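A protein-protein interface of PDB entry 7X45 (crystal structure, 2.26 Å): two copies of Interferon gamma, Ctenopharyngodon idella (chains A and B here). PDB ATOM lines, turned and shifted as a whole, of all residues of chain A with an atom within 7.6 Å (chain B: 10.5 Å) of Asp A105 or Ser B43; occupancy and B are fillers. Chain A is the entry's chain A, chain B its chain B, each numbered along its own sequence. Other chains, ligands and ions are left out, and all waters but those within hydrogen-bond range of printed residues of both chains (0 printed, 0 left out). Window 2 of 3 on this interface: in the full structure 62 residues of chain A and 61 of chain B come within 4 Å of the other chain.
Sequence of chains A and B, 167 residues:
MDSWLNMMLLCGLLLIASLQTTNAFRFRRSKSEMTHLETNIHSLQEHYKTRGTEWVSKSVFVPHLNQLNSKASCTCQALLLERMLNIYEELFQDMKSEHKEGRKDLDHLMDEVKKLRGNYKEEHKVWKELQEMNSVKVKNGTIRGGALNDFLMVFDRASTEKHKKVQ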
ATOM      1  N   PHE A  92      10.379  27.393   3.242  1.00  0.00           N
ATOM      2  CA  PHE A  92       9.671  26.632   4.292  1.00  0.00           C
ATOM      3  C   PHE A  92       9.395  27.617   5.438  1.00  0.00           C
ATOM      4  O   PHE A  92       8.299  27.600   6.003  1.00  0.00           O
ATOM      5  CB  PHE A  92      10.443  25.355   4.653  1.00  0.00           C
ATOM      6  CG  PHE A  92      10.461  24.265   3.596  1.00  0.00           C
ATOM      7  CD1 PHE A  92       9.436  24.131   2.668  1.00  0.00           C
ATOM      8  CD2 PHE A  92      11.490  23.333   3.565  1.00  0.00           C
ATOM      9  CE1 PHE A  92       9.461  23.117   1.714  1.00  0.00           C
ATOM     10  CE2 PHE A  92      11.524  22.332   2.601  1.00  0.00           C
ATOM     11  CZ  PHE A  92      10.509  22.218   1.676  1.00  0.00           C
ATOM     12  N   ARG A 103       3.006  23.007  12.465  1.00  0.00           N
ATOM     13  CA  ARG A 103       2.915  22.137  11.261  1.00  0.00           C
ATOM     14  C   ARG A 103       4.058  21.118  11.291  1.00  0.00           C
ATOM     15  O   ARG A 103       5.200  21.505  10.963  1.00  0.00           O
ATOM     16  CB  ARG A 103       2.966  22.994   9.993  1.00  0.00           C
ATOM     17  CG  ARG A 103       2.504  22.268   8.737  1.00  0.00           C
ATOM     18  CD  ARG A 103       1.026  21.935   8.810  1.00  0.00           C
ATOM     19  NE  ARG A 103       0.207  23.065   9.230  1.00  0.00           N
ATOM     20  CZ  ARG A 103      -0.265  24.021   8.430  1.00  0.00           C
ATOM     21  NH1 ARG A 103       0.000  24.004   7.134  1.00  0.00           N
ATOM     22  NH2 ARG A 103      -1.015  24.988   8.938  1.00  0.00           N
ATOM     23  N   LYS A 104       3.754  19.864  11.650  1.00  0.00           N
ATOM     24  CA  LYS A 104       4.721  18.727  11.712  1.00  0.00           C
ATOM     25  C   LYS A 104       5.454  18.542  10.374  1.00  0.00           C
ATOM     26  O   LYS A 104       6.615  18.069  10.408  1.00  0.00           O
ATOM     27  CB  LYS A 104       4.015  17.418  12.084  1.00  0.00           C
ATOM     28  CG  LYS A 104       2.884  16.981  11.154  1.00  0.00           C
ATOM     29  CD  LYS A 104       2.592  15.496  11.203  1.00  0.00           C
ATOM     30  CE  LYS A 104       1.738  15.025  10.045  1.00  0.00           C
ATOM     31  NZ  LYS A 104       0.365  15.579  10.122  1.00  0.00           N
ATOM     32  N   ASP A 105       4.786  18.865   9.254  1.00  0.00           N
ATOM     33  CA  ASP A 105       5.267  18.735   7.850  1.00  0.00           C
ATOM     34  C   ASP A 105       6.464  19.647   7.597  1.00  0.00           C
ATOM     35  O   ASP A 105       7.575  19.137   7.334  1.00  0.00           O
ATOM     36  CB  ASP A 105       4.200  19.189   6.852  1.00  0.00           C
ATOM     37  CG  ASP A 105       3.010  18.270   6.818  1.00  0.00           C
ATOM     38  OD1 ASP A 105       3.254  17.069   6.884  1.00  0.00           O
ATOM     39  OD2 ASP A 105       1.857  18.772   6.764  1.00  0.00           O
ATOM     40  N   LEU A 106       6.189  20.952   7.656  1.00  0.00           N
ATOM     41  CA  LEU A 106       7.117  22.071   7.362  1.00  0.00           C
ATOM     42  C   LEU A 106       8.338  21.944   8.273  1.00  0.00           C
ATOM     43  O   LEU A 106       9.447  22.214   7.806  1.00  0.00           O
ATOM     44  CB  LEU A 106       6.353  23.378   7.596  1.00  0.00           C
ATOM     45  CG  LEU A 106       6.627  24.524   6.623  1.00  0.00           C
ATOM     46  CD1 LEU A 106       6.852  24.033   5.198  1.00  0.00           C
ATOM     47  CD2 LEU A 106       5.482  25.536   6.641  1.00  0.00           C
ATOM     48  N   ASP A 107       8.120  21.496   9.510  1.00  0.00           N
ATOM     49  CA  ASP A 107       9.145  21.364  10.574  1.00  0.00           C
ATOM     50  C   ASP A 107      10.091  20.213  10.248  1.00  0.00           C
ATOM     51  O   ASP A 107      11.316  20.395  10.408  1.00  0.00           O
ATOM     52  CB  ASP A 107       8.494  21.165  11.945  1.00  0.00           C
ATOM     53  CG  ASP A 107       8.158  22.479  12.635  1.00  0.00           C
ATOM     54  OD1 ASP A 107       8.795  23.495  12.270  1.00  0.00           O
ATOM     55  OD2 ASP A 107       7.275  22.486  13.536  1.00  0.00           O
ATOM     56  N   HIS A 108       9.556  19.056   9.856  1.00  0.00           N
ATOM     57  CA  HIS A 108      10.389  17.867   9.540  1.00  0.00           C
ATOM     58  C   HIS A 108      11.195  18.163   8.274  1.00  0.00           C
ATOM     59  O   HIS A 108      12.337  17.701   8.194  1.00  0.00           O
ATOM     60  CB  HIS A 108       9.570  16.575   9.412  1.00  0.00           C
ATOM     61  CG  HIS A 108      10.437  15.360   9.274  1.00  0.00           C
ATOM     62  ND1 HIS A 108      11.379  15.011  10.231  1.00  0.00           N
ATOM     63  CD2 HIS A 108      10.556  14.443   8.276  1.00  0.00           C
ATOM     64  CE1 HIS A 108      12.024  13.919   9.838  1.00  0.00           C
ATOM     65  NE2 HIS A 108      11.533  13.548   8.641  1.00  0.00           N
ATOM     66  N   LEU A 109      10.617  18.907   7.326  1.00  0.00           N
ATOM     67  CA  LEU A 109      11.282  19.244   6.039  1.00  0.00           C
ATOM     68  C   LEU A 109      12.454  20.189   6.316  1.00  0.00           C
ATOM     69  O   LEU A 109      13.567  19.894   5.845  1.00  0.00           O
ATOM     70  CB  LEU A 109      10.274  19.891   5.084  1.00  0.00           C
ATOM     71  CG  LEU A 109       9.225  18.968   4.486  1.00  0.00           C
ATOM     72  CD1 LEU A 109       8.021  19.776   4.022  1.00  0.00           C
ATOM     73  CD2 LEU A 109       9.818  18.157   3.339  1.00  0.00           C
ATOM     74  N   MET A 110      12.211  21.280   7.049  1.00  0.00           N
ATOM     75  CA  MET A 110      13.274  22.259   7.392  1.00  0.00           C
ATOM     76  C   MET A 110      14.409  21.512   8.107  1.00  0.00           C
ATOM     77  O   MET A 110      15.582  21.779   7.783  1.00  0.00           O
ATOM     78  CB  MET A 110      12.752  23.398   8.281  1.00  0.00           C
ATOM     79  CG  MET A 110      11.717  24.265   7.588  1.00  0.00           C
ATOM     80  SD  MET A 110      11.076  25.619   8.623  1.00  0.00           S
ATOM     81  CE  MET A 110      12.232  26.876   8.084  1.00  0.00           C
ATOM     82  N   ASP A 111      14.071  20.588   9.009  1.00  0.00           N
ATOM     83  CA  ASP A 111      15.065  19.802   9.785  1.00  0.00           C
ATOM     84  C   ASP A 111      15.931  18.968   8.844  1.00  0.00           C
ATOM     85  O   ASP A 111      17.159  18.912   9.078  1.00  0.00           O
ATOM     86  CB  ASP A 111      14.395  18.887  10.810  1.00  0.00           C
ATOM     87  CG  ASP A 111      13.950  19.602  12.065  1.00  0.00           C
ATOM     88  OD1 ASP A 111      14.122  20.833  12.125  1.00  0.00           O
ATOM     89  OD2 ASP A 111      13.428  18.919  12.969  1.00  0.00           O
ATOM     90  N   GLU B  33      13.887   7.327   5.261  1.00  0.00           N
ATOM     91  CA  GLU B  33      13.609   8.758   5.556  1.00  0.00           C
ATOM     92  C   GLU B  33      12.754   9.334   4.413  1.00  0.00           C
ATOM     93  O   GLU B  33      11.845  10.125   4.697  1.00  0.00           O
ATOM     94  CB  GLU B  33      14.948   9.485   5.729  1.00  0.00           C
ATOM     95  CG  GLU B  33      14.826  10.976   6.026  1.00  0.00           C
ATOM     96  CD  GLU B  33      13.925  11.348   7.199  1.00  0.00           C
ATOM     97  OE1 GLU B  33      14.306  11.092   8.368  1.00  0.00           O
ATOM     98  OE2 GLU B  33      12.833  11.888   6.941  1.00  0.00           O
ATOM     99  N   THR B  35      10.380   8.199   2.460  1.00  0.00           N
ATOM    100  CA  THR B  35       8.913   7.954   2.570  1.00  0.00           C
ATOM    101  C   THR B  35       8.275   9.047   3.437  1.00  0.00           C
ATOM    102  O   THR B  35       7.244   9.630   3.031  1.00  0.00           O
ATOM    103  CB  THR B  35       8.631   6.555   3.135  1.00  0.00           C
ATOM    104  OG1 THR B  35       9.385   5.601   2.382  1.00  0.00           O
ATOM    105  CG2 THR B  35       7.163   6.197   3.094  1.00  0.00           C
ATOM    106  N   HIS B  36       8.868   9.298   4.607  1.00  0.00           N
ATOM    107  CA  HIS B  36       8.470  10.384   5.544  1.00  0.00           C
ATOM    108  C   HIS B  36       8.363  11.695   4.754  1.00  0.00           C
ATOM    109  O   HIS B  36       7.288  12.351   4.811  1.00  0.00           O
ATOM    110  CB  HIS B  36       9.464  10.446   6.714  1.00  0.00           C
ATOM    111  CG  HIS B  36       8.948  11.171   7.916  1.00  0.00           C
ATOM    112  ND1 HIS B  36       8.245  12.376   7.822  1.00  0.00           N
ATOM    113  CD2 HIS B  36       9.046  10.897   9.241  1.00  0.00           C
ATOM    114  CE1 HIS B  36       7.946  12.807   9.034  1.00  0.00           C
ATOM    115  NE2 HIS B  36       8.417  11.914   9.918  1.00  0.00           N
ATOM    116  N   LEU B  37       9.417  12.031   3.996  1.00  0.00           N
ATOM    117  CA  LEU B  37       9.508  13.292   3.203  1.00  0.00           C
ATOM    118  C   LEU B  37       8.391  13.326   2.158  1.00  0.00           C
ATOM    119  O   LEU B  37       7.728  14.379   2.050  1.00  0.00           O
ATOM    120  CB  LEU B  37      10.887  13.392   2.540  1.00  0.00           C
ATOM    121  CG  LEU B  37      12.060  13.667   3.484  1.00  0.00           C
ATOM    122  CD1 LEU B  37      13.383  13.505   2.747  1.00  0.00           C
ATOM    123  CD2 LEU B  37      11.955  15.057   4.105  1.00  0.00           C
ATOM    124  N   GLU B  38       8.165  12.210   1.454  1.00  0.00           N
ATOM    125  CA  GLU B  38       7.094  12.091   0.420  1.00  0.00           C
ATOM    126  C   GLU B  38       5.749  12.466   1.044  1.00  0.00           C
ATOM    127  O   GLU B  38       5.016  13.262   0.419  1.00  0.00           O
ATOM    128  CB  GLU B  38       7.045  10.688  -0.182  1.00  0.00           C
ATOM    129  CG  GLU B  38       8.244  10.383  -1.063  1.00  0.00           C
ATOM    130  CD  GLU B  38       8.143   9.106  -1.887  1.00  0.00           C
ATOM    131  OE1 GLU B  38       7.089   8.435  -1.843  1.00  0.00           O
ATOM    132  OE2 GLU B  38       9.140   8.772  -2.558  1.00  0.00           O
ATOM    133  N   THR B  39       5.458  11.922   2.233  1.00  0.00           N
ATOM    134  CA  THR B  39       4.209  12.163   3.008  1.00  0.00           C
ATOM    135  C   THR B  39       4.061  13.658   3.319  1.00  0.00           C
ATOM    136  O   THR B  39       2.955  14.208   3.067  1.00  0.00           O
ATOM    137  CB  THR B  39       4.184  11.329   4.294  1.00  0.00           C
ATOM    138  OG1 THR B  39       4.454   9.971   3.930  1.00  0.00           O
ATOM    139  CG2 THR B  39       2.867  11.435   5.042  1.00  0.00           C
ATOM    140  N   ASN B  40       5.133  14.293   3.823  1.00  0.00           N
ATOM    141  CA  ASN B  40       5.135  15.737   4.187  1.00  0.00           C
ATOM    142  C   ASN B  40       4.822  16.591   2.951  1.00  0.00           C
ATOM    143  O   ASN B  40       3.979  17.486   3.070  1.00  0.00           O
ATOM    144  CB  ASN B  40       6.446  16.178   4.837  1.00  0.00           C
ATOM    145  CG  ASN B  40       6.765  15.465   6.137  1.00  0.00           C
ATOM    146  OD1 ASN B  40       7.921  15.431   6.552  1.00  0.00           O
ATOM    147  ND2 ASN B  40       5.767  14.879   6.777  1.00  0.00           N
ATOM    148  N   ILE B  41       5.456  16.316   1.804  1.00  0.00           N
ATOM    149  CA  ILE B  41       5.266  17.084   0.526  1.00  0.00           C
ATOM    150  C   ILE B  41       3.808  16.966   0.069  1.00  0.00           C
ATOM    151  O   ILE B  41       3.210  18.022  -0.287  1.00  0.00           O
ATOM    152  CB  ILE B  41       6.256  16.619  -0.576  1.00  0.00           C
ATOM    153  CG1 ILE B  41       7.694  17.065  -0.293  1.00  0.00           C
ATOM    154  CG2 ILE B  41       5.810  17.067  -1.956  1.00  0.00           C
ATOM    155  CD1 ILE B  41       7.884  18.563  -0.250  1.00  0.00           C
ATOM    156  N   HIS B  42       3.273  15.738   0.028  1.00  0.00           N
ATOM    157  CA  HIS B  42       1.880  15.451  -0.407  1.00  0.00           C
ATOM    158  C   HIS B  42       0.907  16.271   0.451  1.00  0.00           C
ATOM    159  O   HIS B  42       0.182  17.137  -0.115  1.00  0.00           O
ATOM    160  CB  HIS B  42       1.574  13.943  -0.358  1.00  0.00           C
ATOM    161  CG  HIS B  42       0.193  13.619  -0.828  1.00  0.00           C
ATOM    162  ND1 HIS B  42      -0.193  13.750  -2.162  1.00  0.00           N
ATOM    163  CD2 HIS B  42      -0.909  13.202  -0.161  1.00  0.00           C
ATOM    164  CE1 HIS B  42      -1.466  13.441  -2.286  1.00  0.00           C
ATOM    165  NE2 HIS B  42      -1.925  13.090  -1.080  1.00  0.00           N
ATOM    166  N   SER B  43       0.908  16.022   1.763  1.00  0.00           N
ATOM    167  CA  SER B  43      -0.016  16.662   2.737  1.00  0.00           C
ATOM    168  C   SER B  43       0.114  18.185   2.649  1.00  0.00           C
ATOM    169  O   SER B  43      -0.903  18.882   2.832  1.00  0.00           O
ATOM    170  CB  SER B  43       0.224  16.172   4.142  1.00  0.00           C
ATOM    171  OG  SER B  43       1.543  16.461   4.551  1.00  0.00           O
ATOM    172  N   LEU B  44       1.325  18.667   2.365  1.00  0.00           N
ATOM    173  CA  LEU B  44       1.636  20.114   2.247  1.00  0.00           C
ATOM    174  C   LEU B  44       0.990  20.668   0.972  1.00  0.00           C
ATOM    175  O   LEU B  44       0.421  21.770   1.051  1.00  0.00           O
ATOM    176  CB  LEU B  44       3.161  20.309   2.263  1.00  0.00           C
ATOM    177  CG  LEU B  44       3.650  21.675   2.754  1.00  0.00           C
ATOM    178  CD1 LEU B  44       3.019  22.055   4.084  1.00  0.00           C
ATOM    179  CD2 LEU B  44       5.168  21.698   2.884  1.00  0.00           C
ATOM    180  N   GLN B  45       1.053  19.921  -0.137  1.00  0.00           N
ATOM    181  CA  GLN B  45       0.479  20.314  -1.453  1.00  0.00           C
ATOM    182  C   GLN B  45      -1.048  20.288  -1.388  1.00  0.00           C
ATOM    183  O   GLN B  45      -1.697  21.078  -2.134  1.00  0.00           O
ATOM    184  CB  GLN B  45       0.943  19.362  -2.551  1.00  0.00           C
ATOM    185  CG  GLN B  45       2.322  19.703  -3.069  1.00  0.00           C
ATOM    186  CD  GLN B  45       2.829  18.702  -4.079  1.00  0.00           C
ATOM    187  OE1 GLN B  45       2.751  17.494  -3.880  1.00  0.00           O
ATOM    188  NE2 GLN B  45       3.396  19.216  -5.155  1.00  0.00           N
ATOM    189  N   GLU B  46      -1.587  19.377  -0.571  1.00  0.00           N
ATOM    190  CA  GLU B  46      -3.044  19.277  -0.312  1.00  0.00           C
ATOM    191  C   GLU B  46      -3.505  20.579   0.352  1.00  0.00           C
ATOM    192  O   GLU B  46      -4.506  21.140  -0.121  1.00  0.00           O
ATOM    193  CB  GLU B  46      -3.355  18.016   0.501  1.00  0.00           C
ATOM    194  CG  GLU B  46      -3.160  16.726  -0.292  1.00  0.00           C
ATOM    195  CD  GLU B  46      -3.652  16.727  -1.739  1.00  0.00           C
ATOM    196  OE1 GLU B  46      -4.880  16.834  -1.948  1.00  0.00           O
ATOM    197  OE2 GLU B  46      -2.804  16.619  -2.660  1.00  0.00           O
ATOM    198  N   HIS B  47      -2.785  21.060   1.372  1.00  0.00           N
ATOM    199  CA  HIS B  47      -3.187  22.263   2.159  1.00  0.00           C
ATOM    200  C   HIS B  47      -2.890  23.537   1.353  1.00  0.00           C
ATOM    201  O   HIS B  47      -3.576  24.534   1.618  1.00  0.00           O
ATOM    202  CB  HIS B  47      -2.619  22.253   3.594  1.00  0.00           C
ATOM    203  CG  HIS B  47      -3.570  21.702   4.615  1.00  0.00           C
ATOM    204  ND1 HIS B  47      -3.157  20.871   5.640  1.00  0.00           N
ATOM    205  CD2 HIS B  47      -4.907  21.841   4.775  1.00  0.00           C
ATOM    206  CE1 HIS B  47      -4.192  20.528   6.381  1.00  0.00           C
ATOM    207  NE2 HIS B  47      -5.278  21.106   5.867  1.00  0.00           N
ATOM    208  N   TYR B  48      -1.974  23.500   0.375  1.00  0.00           N
ATOM    209  CA  TYR B  48      -1.643  24.651  -0.514  1.00  0.00           C
ATOM    210  C   TYR B  48      -2.131  24.360  -1.945  1.00  0.00           C
ATOM    211  O   TYR B  48      -1.368  24.570  -2.895  1.00  0.00           O
ATOM    212  CB  TYR B  48      -0.138  24.961  -0.470  1.00  0.00           C
ATOM    213  CG  TYR B  48       0.358  25.702   0.753  1.00  0.00           C
ATOM    214  CD1 TYR B  48       0.679  25.033   1.925  1.00  0.00           C
ATOM    215  CD2 TYR B  48       0.543  27.077   0.729  1.00  0.00           C
ATOM    216  CE1 TYR B  48       1.136  25.711   3.046  1.00  0.00           C
ATOM    217  CE2 TYR B  48       1.013  27.770   1.838  1.00  0.00           C
ATOM    218  CZ  TYR B  48       1.304  27.086   3.008  1.00  0.00           C
ATOM    219  OH  TYR B  48       1.762  27.751   4.112  1.00  0.00           O
ATOM    220  N   LYS B  49      -3.373  23.901  -2.112  1.00  0.00           N
ATOM    221  CA  LYS B  49      -4.043  23.887  -3.437  1.00  0.00           C
ATOM    222  C   LYS B  49      -4.658  25.270  -3.673  1.00  0.00           C
ATOM    223  O   LYS B  49      -4.407  25.817  -4.762  1.00  0.00           O
ATOM    224  CB  LYS B  49      -5.130  22.816  -3.526  1.00  0.00           C
ATOM    225  CG  LYS B  49      -4.669  21.452  -4.021  1.00  0.00           C
ATOM    226  CD  LYS B  49      -5.847  20.602  -4.506  1.00  0.00           C
ATOM    227  CE  LYS B  49      -5.760  19.128  -4.149  1.00  0.00           C
ATOM    228  NZ  LYS B  49      -6.996  18.638  -3.482  1.00  0.00           N
ATOM    229  N   LEU B 148       7.626  22.915  -4.215  1.00  0.00           N
ATOM    230  CA  LEU B 148       7.106  21.688  -3.539  1.00  0.00           C
ATOM    231  C   LEU B 148       7.199  20.470  -4.471  1.00  0.00           C
ATOM    232  O   LEU B 148       7.700  19.427  -4.015  1.00  0.00           O
ATOM    233  CB  LEU B 148       5.665  21.939  -3.091  1.00  0.00           C
ATOM    234  CG  LEU B 148       5.520  22.957  -1.961  1.00  0.00           C
ATOM    235  CD1 LEU B 148       4.054  23.246  -1.667  1.00  0.00           C
ATOM    236  CD2 LEU B 148       6.241  22.482  -0.714  1.00  0.00           C
ATOM    237  N   PHE B 151      11.000  19.305  -4.743  1.00  0.00           N
ATOM    238  CA  PHE B 151      11.779  19.265  -3.482  1.00  0.00           C
ATOM    239  C   PHE B 151      12.563  17.958  -3.403  1.00  0.00           C
ATOM    240  O   PHE B 151      13.773  17.971  -3.040  1.00  0.00           O
ATOM    241  CB  PHE B 151      10.927  19.373  -2.216  1.00  0.00           C
ATOM    242  CG  PHE B 151      11.755  19.112  -0.978  1.00  0.00           C
ATOM    243  CD1 PHE B 151      12.646  20.066  -0.520  1.00  0.00           C
ATOM    244  CD2 PHE B 151      11.739  17.874  -0.354  1.00  0.00           C
ATOM    245  CE1 PHE B 151      13.449  19.822   0.580  1.00  0.00           C
ATOM    246  CE2 PHE B 151      12.560  17.619   0.733  1.00  0.00           C
ATOM    247  CZ  PHE B 151      13.407  18.596   1.204  1.00  0.00           C
ATOM    248  N   LEU B 152      11.880  16.850  -3.671  1.00  0.00           N
ATOM    249  CA  LEU B 152      12.456  15.503  -3.458  1.00  0.00           C
ATOM    250  C   LEU B 152      13.545  15.285  -4.505  1.00  0.00           C
ATOM    251  O   LEU B 152      14.571  14.709  -4.154  1.00  0.00           O
ATOM    252  CB  LEU B 152      11.333  14.460  -3.508  1.00  0.00           C
ATOM    253  CG  LEU B 152      10.229  14.698  -2.472  1.00  0.00           C
ATOM    254  CD1 LEU B 152       8.930  14.019  -2.888  1.00  0.00           C
ATOM    255  CD2 LEU B 152      10.674  14.236  -1.099  1.00  0.00           C
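O of Thr B39 lies within hydrogen-bond range of OG of Ser B43, at 3.0 Å. ND1 of His B36 sits at hydrogen-bond distance from OD1 of Asn B40 (3.3 Å). O of Asn B40 is in hydrogen-bond range of OG of Ser B43 (3.0 Å).
No position is printed for both chains.
Of the printed residues of chain B, Phe A92 touches Phe B151. Printed residues of chain B within 4 Å of Asp A105: Asn B40 and Ser B43. Leu A106 touches just one residue of chain B: Leu B44. Of chain B, only Leu B37 (3.8 Å), Asn B40 (3.95 Å), Leu B44 (3.6 Å) and Phe B151 (3.8 Å) come within 4 Å of Leu A109. Of the printed residues of chain A, Glu B33 touches His A108 (2.7 Å). Of the printed residues of chain A, Leu B37 touches Leu A109 (3.8 Å). Ser B43 touches just one residue of chain A: Asp A105. Of the printed residues of chain A, Leu B44 touches Leu A106 and Leu A109. Leu B148 touches none of the printed residues of chain A. Printed residues of chain A within 4 Å of Phe B151: Phe A92 (3.7 Å) and Leu A109 (3.8 Å). The nearest residue of chain B that does not touch Asp A105 is Leu B44 (4.2 Å). The nearest residue of chain A that does not touch Ser B43 is Lys A104 (5.7 Å). The nearest printed residue of chain A that does not touch Asn B40 is Lys A104 (4.9 Å).
The side-chain hydroxyl (OG) of Ser B43 is in hydrogen-bond range of the side-chain carboxylate (OD1) of Asp A105, 3.0 Å away. OD1 of Asp A105 sits at hydrogen-bond distance from ND2 of Asn B40, 3.3 Å away. NE2 of His A108 is in hydrogen-bond range of OE2 of Glu B33 (2.7 Å).
Of the 19 printed residues of chain B, 7 touch a printed residue of chain A. Printed residues of chain B that touch a printed residue of chain A: Glu B33, His B36, Leu B37, Asn B40, Ser B43, Leu B44 and Phe B151. Among the printed residues, no Asp or Glu carboxylate lies within 4 Å of a Lys or Arg side-chain nitrogen of the other chain.
Among the printed residues, merely in contact across the chains: Phe A92 with Phe B151 (3.7 Å), Leu A106 with Leu B44 (3.7 Å), His A108 with His B36 (3.1 Å), His A108 with Asn B40 (3.3 Å), Leu A109 with Leu B37 (3.8 Å), Leu A109 with Asn B40 (3.95 Å), Leu A109 with Leu B44 (3.6 Å) and Leu A109 with Phe B151 (3.8 Å).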
